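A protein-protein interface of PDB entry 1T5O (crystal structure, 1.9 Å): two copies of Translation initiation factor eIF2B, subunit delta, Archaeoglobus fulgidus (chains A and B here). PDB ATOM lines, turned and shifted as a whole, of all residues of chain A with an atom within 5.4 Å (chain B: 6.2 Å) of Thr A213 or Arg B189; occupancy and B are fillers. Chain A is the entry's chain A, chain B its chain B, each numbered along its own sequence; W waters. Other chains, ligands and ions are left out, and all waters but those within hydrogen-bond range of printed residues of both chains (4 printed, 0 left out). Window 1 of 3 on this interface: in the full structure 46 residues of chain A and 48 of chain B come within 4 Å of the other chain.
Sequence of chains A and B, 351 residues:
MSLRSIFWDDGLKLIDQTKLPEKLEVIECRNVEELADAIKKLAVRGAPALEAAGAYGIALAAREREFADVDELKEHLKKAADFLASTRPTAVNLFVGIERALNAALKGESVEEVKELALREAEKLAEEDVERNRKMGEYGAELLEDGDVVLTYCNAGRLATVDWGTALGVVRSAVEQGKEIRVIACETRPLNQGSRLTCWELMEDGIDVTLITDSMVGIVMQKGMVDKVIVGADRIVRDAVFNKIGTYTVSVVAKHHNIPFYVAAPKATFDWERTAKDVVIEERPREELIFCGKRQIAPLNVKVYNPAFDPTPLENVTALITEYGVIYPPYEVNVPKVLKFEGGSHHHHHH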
ATOM      1  N   CYS A 186      24.327   8.682 -15.628  1.00  0.00           N
ATOM      2  CA  CYS A 186      23.888   7.329 -15.985  1.00  0.00           C
ATOM      3  C   CYS A 186      22.527   7.427 -16.652  1.00  0.00           C
ATOM      4  O   CYS A 186      21.659   8.141 -16.148  1.00  0.00           O
ATOM      5  CB  CYS A 186      23.788   6.469 -14.727  1.00  0.00           C
ATOM      6  SG  CYS A 186      25.425   6.158 -14.090  1.00  0.00           S
ATOM      7  N   GLU A 187      22.324   6.700 -17.758  1.00  0.00           N
ATOM      8  CA  GLU A 187      21.069   6.798 -18.495  1.00  0.00           C
ATOM      9  C   GLU A 187      19.869   6.509 -17.612  1.00  0.00           C
ATOM     10  O   GLU A 187      18.809   7.078 -17.820  1.00  0.00           O
ATOM     11  CB  GLU A 187      21.071   5.892 -19.740  1.00  0.00           C
ATOM     12  CG  GLU A 187      20.833   4.425 -19.460  1.00  0.00           C
ATOM     13  CD  GLU A 187      20.758   3.582 -20.739  1.00  0.00           C
ATOM     14  OE1 GLU A 187      20.282   4.090 -21.784  1.00  0.00           O
ATOM     15  OE2 GLU A 187      21.155   2.394 -20.683  1.00  0.00           O
ATOM     16  N   ARG A 189      18.106   3.185 -16.476  1.00  0.00           N
ATOM     17  CA  ARG A 189      17.050   2.306 -16.988  1.00  0.00           C
ATOM     18  C   ARG A 189      16.020   2.033 -15.872  1.00  0.00           C
ATOM     19  O   ARG A 189      16.320   2.233 -14.715  1.00  0.00           O
ATOM     20  CB  ARG A 189      17.680   1.003 -17.482  1.00  0.00           C
ATOM     21  CG  ARG A 189      18.518   1.214 -18.750  1.00  0.00           C
ATOM     22  CD  ARG A 189      17.610   1.475 -19.909  1.00  0.00           C
ATOM     23  NE  ARG A 189      16.833   0.270 -20.213  1.00  0.00           N
ATOM     24  CZ  ARG A 189      15.724   0.258 -20.945  1.00  0.00           C
ATOM     25  NH1 ARG A 189      15.238   1.390 -21.452  1.00  0.00           N
ATOM     26  NH2 ARG A 189      15.101  -0.890 -21.175  1.00  0.00           N
ATOM     27  N   ASN A 192      14.902   5.783 -18.385  1.00  0.00           N
ATOM     28  CA  ASN A 192      15.895   6.733 -18.898  1.00  0.00           C
ATOM     29  C   ASN A 192      15.793   8.186 -18.455  1.00  0.00           C
ATOM     30  O   ASN A 192      15.950   9.117 -19.274  1.00  0.00           O
ATOM     31  CB  ASN A 192      15.910   6.713 -20.425  1.00  0.00           C
ATOM     32  CG  ASN A 192      16.531   5.457 -20.970  1.00  0.00           C
ATOM     33  OD1 ASN A 192      15.960   4.354 -20.850  1.00  0.00           O
ATOM     34  ND2 ASN A 192      17.718   5.596 -21.556  1.00  0.00           N
ATOM     35  N   LEU A 211      27.133  11.095 -21.171  1.00  0.00           N
ATOM     36  CA  LEU A 211      26.113  10.053 -20.981  1.00  0.00           C
ATOM     37  C   LEU A 211      26.739   8.677 -21.068  1.00  0.00           C
ATOM     38  O   LEU A 211      27.501   8.396 -21.996  1.00  0.00           O
ATOM     39  CB  LEU A 211      25.076  10.168 -22.103  1.00  0.00           C
ATOM     40  CG  LEU A 211      23.580   9.827 -21.976  1.00  0.00           C
ATOM     41  CD1 LEU A 211      23.092   9.308 -23.283  1.00  0.00           C
ATOM     42  CD2 LEU A 211      23.295   8.853 -20.871  1.00  0.00           C
ATOM     43  N   ILE A 212      26.412   7.816 -20.107  1.00  0.00           N
ATOM     44  CA  ILE A 212      26.934   6.437 -20.087  1.00  0.00           C
ATOM     45  C   ILE A 212      25.802   5.552 -19.671  1.00  0.00           C
ATOM     46  O   ILE A 212      24.783   6.044 -19.188  1.00  0.00           O
ATOM     47  CB  ILE A 212      28.051   6.214 -19.026  1.00  0.00           C
ATOM     48  CG1 ILE A 212      27.545   6.535 -17.597  1.00  0.00           C
ATOM     49  CG2 ILE A 212      29.240   7.058 -19.348  1.00  0.00           C
ATOM     50  CD1 ILE A 212      28.559   6.116 -16.499  1.00  0.00           C
ATOM     51  N   THR A 213      25.962   4.249 -19.884  1.00  0.00           N
ATOM     52  CA  THR A 213      24.950   3.306 -19.457  1.00  0.00           C
ATOM     53  C   THR A 213      25.145   3.160 -17.920  1.00  0.00           C
ATOM     54  O   THR A 213      26.205   3.527 -17.381  1.00  0.00           O
ATOM     55  CB  THR A 213      25.180   1.958 -20.195  1.00  0.00           C
ATOM     56  OG1 THR A 213      24.037   1.135 -20.055  1.00  0.00           O
ATOM     57  CG2 THR A 213      26.347   1.252 -19.640  1.00  0.00           C
ATOM     58  N   ASP A 214      24.147   2.640 -17.213  1.00  0.00           N
ATOM     59  CA  ASP A 214      24.279   2.450 -15.755  1.00  0.00           C
ATOM     60  C   ASP A 214      25.395   1.468 -15.412  1.00  0.00           C
ATOM     61  O   ASP A 214      26.139   1.652 -14.434  1.00  0.00           O
ATOM     62  CB  ASP A 214      22.950   1.928 -15.152  1.00  0.00           C
ATOM     63  CG  ASP A 214      21.772   2.773 -15.559  1.00  0.00           C
ATOM     64  OD1 ASP A 214      21.947   4.002 -15.613  1.00  0.00           O
ATOM     65  OD2 ASP A 214      20.680   2.216 -15.814  1.00  0.00           O
ATOM     66  N   SER A 215      25.515   0.436 -16.236  1.00  0.00           N
ATOM     67  CA  SER A 215      26.517  -0.595 -16.050  1.00  0.00           C
ATOM     68  C   SER A 215      27.946  -0.061 -16.212  1.00  0.00           C
ATOM     69  O   SER A 215      28.909  -0.704 -15.757  1.00  0.00           O
ATOM     70  CB  SER A 215      26.300  -1.724 -17.066  1.00  0.00           C
ATOM     71  OG  SER A 215      26.700  -1.273 -18.363  1.00  0.00           O
ATOM     72  N   MET A 216      28.100   1.093 -16.867  1.00  0.00           N
ATOM     73  CA  MET A 216      29.440   1.661 -17.073  1.00  0.00           C
ATOM     74  C   MET A 216      29.978   2.339 -15.829  1.00  0.00           C
ATOM     75  O   MET A 216      31.090   2.860 -15.841  1.00  0.00           O
ATOM     76  CB  MET A 216      29.444   2.672 -18.239  1.00  0.00           C
ATOM     77  CG  MET A 216      29.493   2.022 -19.608  1.00  0.00           C
ATOM     78  SD  MET A 216      28.934   3.138 -20.924  1.00  0.00           S
ATOM     79  CE  MET A 216      28.596   1.990 -22.236  1.00  0.00           C
ATOM     80  N   VAL A 217      29.208   2.349 -14.751  1.00  0.00           N
ATOM     81  CA  VAL A 217      29.689   2.964 -13.528  1.00  0.00           C
ATOM     82  C   VAL A 217      30.988   2.268 -13.096  1.00  0.00           C
ATOM     83  O   VAL A 217      31.865   2.896 -12.534  1.00  0.00           O
ATOM     84  CB  VAL A 217      28.646   2.843 -12.377  1.00  0.00           C
ATOM     85  CG1 VAL A 217      29.182   3.516 -11.110  1.00  0.00           C
ATOM     86  CG2 VAL A 217      27.347   3.543 -12.806  1.00  0.00           C
ATOM     87  N   CYS A 292      10.905  -0.690 -26.011  1.00  0.00           N
ATOM     88  CA  CYS A 292      11.676   0.544 -25.873  1.00  0.00           C
ATOM     89  C   CYS A 292      11.244   1.385 -27.054  1.00  0.00           C
ATOM     90  O   CYS A 292      11.664   1.146 -28.191  1.00  0.00           O
ATOM     91  CB  CYS A 292      13.173   0.307 -25.932  1.00  0.00           C
ATOM     92  SG  CYS A 292      13.994   1.658 -25.077  1.00  0.00           S
ATOM     93  N   TYR B 153      25.011 -12.319 -17.649  1.00  0.00           N
ATOM     94  CA  TYR B 153      25.171 -11.022 -18.270  1.00  0.00           C
ATOM     95  C   TYR B 153      25.380 -11.229 -19.770  1.00  0.00           C
ATOM     96  O   TYR B 153      25.934 -12.246 -20.185  1.00  0.00           O
ATOM     97  CB  TYR B 153      26.375 -10.294 -17.677  1.00  0.00           C
ATOM     98  CG  TYR B 153      26.208  -8.788 -17.753  1.00  0.00           C
ATOM     99  CD1 TYR B 153      25.330  -8.133 -16.887  1.00  0.00           C
ATOM    100  CD2 TYR B 153      26.870  -8.037 -18.721  1.00  0.00           C
ATOM    101  CE1 TYR B 153      25.114  -6.779 -16.981  1.00  0.00           C
ATOM    102  CE2 TYR B 153      26.662  -6.656 -18.819  1.00  0.00           C
ATOM    103  CZ  TYR B 153      25.784  -6.047 -17.948  1.00  0.00           C
ATOM    104  OH  TYR B 153      25.559  -4.696 -18.002  1.00  0.00           O
ATOM    105  N   CYS B 186      20.420  -9.997 -16.955  1.00  0.00           N
ATOM    106  CA  CYS B 186      20.499  -8.532 -17.052  1.00  0.00           C
ATOM    107  C   CYS B 186      20.262  -8.163 -18.520  1.00  0.00           C
ATOM    108  O   CYS B 186      20.876  -8.782 -19.403  1.00  0.00           O
ATOM    109  CB  CYS B 186      21.878  -8.074 -16.638  1.00  0.00           C
ATOM    110  SG  CYS B 186      22.215  -8.405 -14.911  1.00  0.00           S
ATOM    111  N   GLU B 187      19.418  -7.153 -18.782  1.00  0.00           N
ATOM    112  CA  GLU B 187      19.102  -6.763 -20.164  1.00  0.00           C
ATOM    113  C   GLU B 187      20.338  -6.478 -21.000  1.00  0.00           C
ATOM    114  O   GLU B 187      20.308  -6.644 -22.225  1.00  0.00           O
ATOM    115  CB  GLU B 187      18.148  -5.540 -20.216  1.00  0.00           C
ATOM    116  CG  GLU B 187      18.753  -4.218 -19.790  1.00  0.00           C
ATOM    117  CD  GLU B 187      17.779  -3.040 -19.909  1.00  0.00           C
ATOM    118  OE1 GLU B 187      18.028  -2.012 -19.262  1.00  0.00           O
ATOM    119  OE2 GLU B 187      16.779  -3.129 -20.651  1.00  0.00           O
ATOM    120  N   THR B 188      21.408  -6.036 -20.343  1.00  0.00           N
ATOM    121  CA  THR B 188      22.702  -5.738 -20.978  1.00  0.00           C
ATOM    122  C   THR B 188      22.681  -4.556 -21.982  1.00  0.00           C
ATOM    123  O   THR B 188      22.723  -4.742 -23.199  1.00  0.00           O
ATOM    124  CB  THR B 188      23.274  -6.967 -21.693  1.00  0.00           C
ATOM    125  OG1 THR B 188      23.175  -8.113 -20.847  1.00  0.00           O
ATOM    126  CG2 THR B 188      24.755  -6.742 -22.024  1.00  0.00           C
ATOM    127  N   ARG B 189      22.607  -3.335 -21.455  1.00  0.00           N
ATOM    128  CA  ARG B 189      22.615  -2.134 -22.293  1.00  0.00           C
ATOM    129  C   ARG B 189      24.007  -1.972 -22.920  1.00  0.00           C
ATOM    130  O   ARG B 189      24.985  -2.525 -22.398  1.00  0.00           O
ATOM    131  CB  ARG B 189      22.237  -0.912 -21.428  1.00  0.00           C
ATOM    132  CG  ARG B 189      20.755  -0.935 -21.039  1.00  0.00           C
ATOM    133  CD  ARG B 189      19.871  -0.672 -22.240  1.00  0.00           C
ATOM    134  NE  ARG B 189      20.049   0.713 -22.673  1.00  0.00           N
ATOM    135  CZ  ARG B 189      19.626   1.210 -23.829  1.00  0.00           C
ATOM    136  NH1 ARG B 189      18.996   0.433 -24.700  1.00  0.00           N
ATOM    137  NH2 ARG B 189      19.807   2.503 -24.092  1.00  0.00           N
ATOM    138  N   PRO B 190      24.116  -1.230 -24.052  1.00  0.00           N
ATOM    139  CA  PRO B 190      23.006  -0.554 -24.730  1.00  0.00           C
ATOM    140  C   PRO B 190      22.380  -1.330 -25.903  1.00  0.00           C
ATOM    141  O   PRO B 190      21.430  -0.842 -26.510  1.00  0.00           O
ATOM    142  CB  PRO B 190      23.651   0.740 -25.211  1.00  0.00           C
ATOM    143  CG  PRO B 190      24.984   0.255 -25.679  1.00  0.00           C
ATOM    144  CD  PRO B 190      25.407  -0.720 -24.557  1.00  0.00           C
ATOM    145  N   LEU B 191      22.906  -2.507 -26.244  1.00  0.00           N
ATOM    146  CA  LEU B 191      22.341  -3.251 -27.365  1.00  0.00           C
ATOM    147  C   LEU B 191      21.335  -4.323 -26.932  1.00  0.00           C
ATOM    148  O   LEU B 191      20.707  -4.978 -27.771  1.00  0.00           O
ATOM    149  CB  LEU B 191      23.462  -3.875 -28.243  1.00  0.00           C
ATOM    150  CG  LEU B 191      24.293  -2.890 -29.074  1.00  0.00           C
ATOM    151  CD1 LEU B 191      25.124  -3.670 -30.099  1.00  0.00           C
ATOM    152  CD2 LEU B 191      23.353  -1.890 -29.822  1.00  0.00           C
ATOM    153  N   ASN B 192      21.177  -4.481 -25.621  1.00  0.00           N
ATOM    154  CA  ASN B 192      20.220  -5.418 -25.056  1.00  0.00           C
ATOM    155  C   ASN B 192      20.369  -6.879 -25.450  1.00  0.00           C
ATOM    156  O   ASN B 192      19.377  -7.557 -25.724  1.00  0.00           O
ATOM    157  CB  ASN B 192      18.790  -4.950 -25.372  1.00  0.00           C
ATOM    158  CG  ASN B 192      18.354  -3.804 -24.497  1.00  0.00           C
ATOM    159  OD1 ASN B 192      18.837  -2.677 -24.649  1.00  0.00           O
ATOM    160  ND2 ASN B 192      17.443  -4.086 -23.550  1.00  0.00           N
ATOM    161  N   GLN B 193      21.597  -7.380 -25.472  1.00  0.00           N
ATOM    162  CA  GLN B 193      21.785  -8.782 -25.813  1.00  0.00           C
ATOM    163  C   GLN B 193      21.081  -9.661 -24.778  1.00  0.00           C
ATOM    164  O   GLN B 193      20.686 -10.790 -25.080  1.00  0.00           O
ATOM    165  CB  GLN B 193      23.267  -9.163 -25.835  1.00  0.00           C
ATOM    166  CG  GLN B 193      24.043  -8.635 -27.027  1.00  0.00           C
ATOM    167  CD  GLN B 193      24.628  -7.257 -26.762  1.00  0.00           C
ATOM    168  OE1 GLN B 193      24.232  -6.571 -25.817  1.00  0.00           O
ATOM    169  NE2 GLN B 193      25.560  -6.837 -27.607  1.00  0.00           N
ATOM    170  N   ASP B 214      20.319  -3.845 -15.826  1.00  0.00           N
ATOM    171  CA  ASP B 214      21.683  -4.098 -15.359  1.00  0.00           C
ATOM    172  C   ASP B 214      21.891  -3.532 -13.962  1.00  0.00           C
ATOM    173  O   ASP B 214      22.597  -4.119 -13.147  1.00  0.00           O
ATOM    174  CB  ASP B 214      22.704  -3.454 -16.313  1.00  0.00           C
ATOM    175  CG  ASP B 214      22.549  -3.927 -17.758  1.00  0.00           C
ATOM    176  OD1 ASP B 214      22.760  -3.092 -18.686  1.00  0.00           O
ATOM    177  OD2 ASP B 214      22.228  -5.131 -17.958  1.00  0.00           O
ATOM    178  N   LYS B 244      31.620  -8.224 -22.302  1.00  0.00           N
ATOM    179  CA  LYS B 244      30.671  -7.141 -22.541  1.00  0.00           C
ATOM    180  C   LYS B 244      30.651  -6.122 -21.398  1.00  0.00           C
ATOM    181  O   LYS B 244      30.539  -6.483 -20.220  1.00  0.00           O
ATOM    182  CB  LYS B 244      29.269  -7.702 -22.762  1.00  0.00           C
ATOM    183  CG  LYS B 244      28.240  -6.609 -23.109  1.00  0.00           C
ATOM    184  CD  LYS B 244      28.649  -5.798 -24.359  1.00  0.00           C
ATOM    185  CE  LYS B 244      28.855  -6.667 -25.597  1.00  0.00           C
ATOM    186  NZ  LYS B 244      29.384  -5.802 -26.726  1.00  0.00           N
ATOM    187  N   ILE B 245      30.746  -4.847 -21.762  1.00  0.00           N
ATOM    188  CA  ILE B 245      30.756  -3.732 -20.808  1.00  0.00           C
ATOM    189  C   ILE B 245      29.636  -3.945 -19.790  1.00  0.00           C
ATOM    190  O   ILE B 245      28.498  -4.255 -20.163  1.00  0.00           O
ATOM    191  CB  ILE B 245      30.560  -2.378 -21.559  1.00  0.00           C
ATOM    192  CG1 ILE B 245      30.540  -1.210 -20.579  1.00  0.00           C
ATOM    193  CG2 ILE B 245      29.239  -2.404 -22.372  1.00  0.00           C
ATOM    194  CD1 ILE B 245      31.921  -0.911 -19.916  1.00  0.00           C
ATOM    195  N   GLU B 288      23.863   4.492 -30.133  1.00  0.00           N
ATOM    196  CA  GLU B 288      23.339   3.396 -29.318  1.00  0.00           C
ATOM    197  C   GLU B 288      22.783   3.909 -27.993  1.00  0.00           C
ATOM    198  O   GLU B 288      21.943   3.254 -27.383  1.00  0.00           O
ATOM    199  CB  GLU B 288      24.428   2.347 -29.055  1.00  0.00           C
ATOM    200  CG  GLU B 288      24.915   1.651 -30.329  1.00  0.00           C
ATOM    201  CD  GLU B 288      25.925   0.563 -30.057  1.00  0.00           C
ATOM    202  OE1 GLU B 288      26.294   0.355 -28.881  1.00  0.00           O
ATOM    203  OE2 GLU B 288      26.355  -0.091 -31.028  1.00  0.00           O
ATOM    204  N   LEU B 289      23.252   5.071 -27.546  1.00  0.00           N
ATOM    205  CA  LEU B 289      22.749   5.669 -26.294  1.00  0.00           C
ATOM    206  C   LEU B 289      21.737   6.814 -26.549  1.00  0.00           C
ATOM    207  O   LEU B 289      21.071   7.289 -25.633  1.00  0.00           O
ATOM    208  CB  LEU B 289      23.898   6.269 -25.467  1.00  0.00           C
ATOM    209  CG  LEU B 289      25.121   5.515 -24.916  1.00  0.00           C
ATOM    210  CD1 LEU B 289      25.116   5.666 -23.403  1.00  0.00           C
ATOM    211  CD2 LEU B 289      25.133   4.059 -25.317  1.00  0.00           C
ATOM    212  N   PHE B 291      19.277   6.808 -29.161  1.00  0.00           N
ATOM    213  CA  PHE B 291      17.997   6.336 -29.687  1.00  0.00           C
ATOM    214  C   PHE B 291      17.683   4.920 -29.250  1.00  0.00           C
ATOM    215  O   PHE B 291      18.579   4.108 -29.028  1.00  0.00           O
ATOM    216  CB  PHE B 291      18.010   6.348 -31.231  1.00  0.00           C
ATOM    217  CG  PHE B 291      17.838   7.720 -31.843  1.00  0.00           C
ATOM    218  CD1 PHE B 291      16.569   8.264 -32.014  1.00  0.00           C
ATOM    219  CD2 PHE B 291      18.948   8.476 -32.208  1.00  0.00           C
ATOM    220  CE1 PHE B 291      16.404   9.557 -32.540  1.00  0.00           C
ATOM    221  CE2 PHE B 291      18.799   9.768 -32.734  1.00  0.00           C
ATOM    222  CZ  PHE B 291      17.524  10.303 -32.896  1.00  0.00           C
ATOM    223  N   CYS B 292      16.386   4.643 -29.147  1.00  0.00           N
ATOM    224  CA  CYS B 292      15.880   3.325 -28.818  1.00  0.00           C
ATOM    225  C   CYS B 292      14.757   3.095 -29.809  1.00  0.00           C
ATOM    226  O   CYS B 292      13.725   3.767 -29.760  1.00  0.00           O
ATOM    227  CB  CYS B 292      15.359   3.275 -27.404  1.00  0.00           C
ATOM    228  SG  CYS B 292      15.986   1.802 -26.676  1.00  0.00           S
ATOM    229  N   ILE B 297      16.063   9.254 -26.995  1.00  0.00           N
ATOM    230  CA  ILE B 297      16.118   9.139 -25.533  1.00  0.00           C
ATOM    231  C   ILE B 297      17.181  10.028 -24.909  1.00  0.00           C
ATOM    232  O   ILE B 297      17.345  10.058 -23.693  1.00  0.00           O
ATOM    233  CB  ILE B 297      16.355   7.660 -25.073  1.00  0.00           C
ATOM    234  CG1 ILE B 297      17.685   7.137 -25.632  1.00  0.00           C
ATOM    235  CG2 ILE B 297      15.168   6.802 -25.493  1.00  0.00           C
ATOM    236  CD1 ILE B 297      18.091   5.707 -25.127  1.00  0.00           C
ATOM    237  N   TYR B 305      29.968   8.270 -23.879  1.00  0.00           N
ATOM    238  CA  TYR B 305      31.100   7.395 -23.623  1.00  0.00           C
ATOM    239  C   TYR B 305      30.453   5.979 -23.748  1.00  0.00           C
ATOM    240  O   TYR B 305      29.575   5.585 -22.942  1.00  0.00           O
ATOM    241  CB  TYR B 305      31.702   7.641 -22.228  1.00  0.00           C
ATOM    242  CG  TYR B 305      32.860   6.711 -21.893  1.00  0.00           C
ATOM    243  CD1 TYR B 305      33.923   6.519 -22.783  1.00  0.00           C
ATOM    244  CD2 TYR B 305      32.862   5.979 -20.707  1.00  0.00           C
ATOM    245  CE1 TYR B 305      34.953   5.608 -22.498  1.00  0.00           C
ATOM    246  CE2 TYR B 305      33.876   5.087 -20.408  1.00  0.00           C
ATOM    247  CZ  TYR B 305      34.917   4.902 -21.302  1.00  0.00           C
ATOM    248  OH  TYR B 305      35.913   4.016 -20.970  1.00  0.00           O
ATOM    249  N   ASN B 306      30.856   5.247 -24.783  1.00  0.00           N
ATOM    250  CA  ASN B 306      30.289   3.929 -25.057  1.00  0.00           C
ATOM    251  C   ASN B 306      31.292   2.789 -25.313  1.00  0.00           C
ATOM    252  O   ASN B 306      31.332   2.211 -26.413  1.00  0.00           O
ATOM    253  CB  ASN B 306      29.321   4.062 -26.248  1.00  0.00           C
ATOM    254  CG  ASN B 306      28.403   2.855 -26.411  1.00  0.00           C
ATOM    255  OD1 ASN B 306      28.170   2.116 -25.470  1.00  0.00           O
ATOM    256  ND2 ASN B 306      27.850   2.679 -27.606  1.00  0.00           N
HETATM  257  O   HOH W   1      20.206  -0.448 -15.782  1.00  0.00           O
HETATM  258  O   HOH W   2      23.520  -0.598 -18.175  1.00  0.00           O
HETATM  259  O   HOH W   3      26.017  -3.480 -20.130  1.00  0.00           O
HETATM  260  O   HOH W   4      20.805   6.693 -23.114  1.00  0.00           O
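The side-chain carboxylate of Glu A187 is in salt-bridge range of the guanidinium group of Arg B189, at 2.8 Å. The side-chain carboxylate (OE1) of Glu B187 is in salt-bridge range of the guanidinium group (NE) of Arg A189, 2.7 Å away. O of Leu A211 is in hydrogen-bond range of N of Tyr B305, at 3.1 Å. The side-chain sulfur of Met A216 sits close to the backbone carbonyl oxygen of Tyr B305 (3.2 Å). The side-chain sulfur of Cys A292 lies close to the side-chain sulfur of Cys B292 (2.6 Å).
The backbone NH of Glu A187 sits at hydrogen-bond distance from the backbone carbonyl oxygen of Ile A212. NH1 of Arg A189 is in hydrogen-bond range of OD1 of Asn A192 (3.1 Å). OD2 of Asp A214 is in hydrogen-bond range of N of Arg A189. The side-chain hydroxyl of Tyr B153 sits close to the side-chain carboxylate of Asp B214. NH1 of Arg B189 sits at hydrogen-bond distance from OD1 of Asn B192 (3.1 Å). The side-chain carboxylate (OD1) of Asp B214 lies within hydrogen-bond range of the backbone NH (N) of Arg B189, 2.8 Å away.
Among the printed residues, merely in contact across the chains: Arg A189 with Arg B189 (3.8 Å), Asn A192 with Ile B297 (3.6 Å), Leu A211 with Leu B289 (3.7 Å), Ile A212 with Leu B289 (3.8 Å), Ile A212 with Tyr B305 (3.8 Å), Thr A213 with Arg B189 (3.1 Å), Thr A213 with Leu B289 (3.9 Å), Ser A215 with Tyr B153 (3.2 Å), Ser A215 with Ile B245 (3.9 Å), Met A216 with Ile B245 (3.5 Å) and Met A216 with Asn B306 (3.3 Å).
Of the printed residues of chain B, Glu A187 touches Arg B189. Printed residues of chain B within 4 Å of Asn A192: Ile B297. Of chain B, only Arg B189 (3.1 Å) and Leu B289 (3.9 Å) come within 4 Å of Thr A213. Printed residues of chain B within 4 Å of Ser A215: Tyr B153 (3.2 Å) and Ile B245 (3.9 Å). Printed residues of chain A within 4 Å of Arg B189: Glu A187, Arg A189 and Thr A213. Gln B193 touches none of the printed residues of chain A. Printed residues of chain A within 4 Å of Ile B245: Ser A215 (3.9 Å) and Met A216 (3.5 Å). Printed residues of chain A within 4 Å of Leu B289: Leu A211 (3.7 Å), Ile A212 (3.8 Å) and Thr A213 (3.9 Å). The nearest printed residue of chain B that does not touch Ile A212 is Asn B306 (6.0 Å).
Hydrophobic or aromatic side chains of chain A within 4 Å of the printed part of chain B: Leu A211, Ile A212 and Met A216. Of the 19 printed residues of chain B, 9 touch a printed residue of chain A. Hydrophobic or aromatic side chains of chain B within 4 Å of the printed part of chain A: Tyr B153, Ile B245, Leu B289, Ile B297 and Tyr B305. Among the printed residues, 16 pairs touch across the chains. Among the printed residues, Asp or Glu carboxylates within 4 Å of a Lys or Arg side-chain nitrogen of the other chain: Glu A187 with Arg B189 (2.8 Å) and Arg A189 with Glu B187 (2.7 Å).
Glu A187 touches Arg B189, and with the chains exchanged Arg A189 touches Glu B187. Arg A189 touches its own counterpart, Arg B189. Cys A292 touches its own counterpart, Cys B292. 6 positions are printed for both chains.
Water W3 lies within hydrogen-bond range of OH of Tyr B153 (2.5 Å), O of Ile B245 (2.6 Å), O of Arg B189 (2.7 Å) and OG of Ser A215 (2.9 Å). Water W4 bridges the backbone carbonyl oxygen of Leu B289 (2.6 Å) and the side-chain carboxylate of Glu A187 (3.0 Å). Water W2 lies within hydrogen-bond range of OG1 of Thr A213, OD1 of Asp B214, N of Ser A215 and N of Asp A214. Water W1 lies within hydrogen-bond range of OD2 of Asp A214 (2.7 Å) and N of Asp B214 (3.4 Å).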
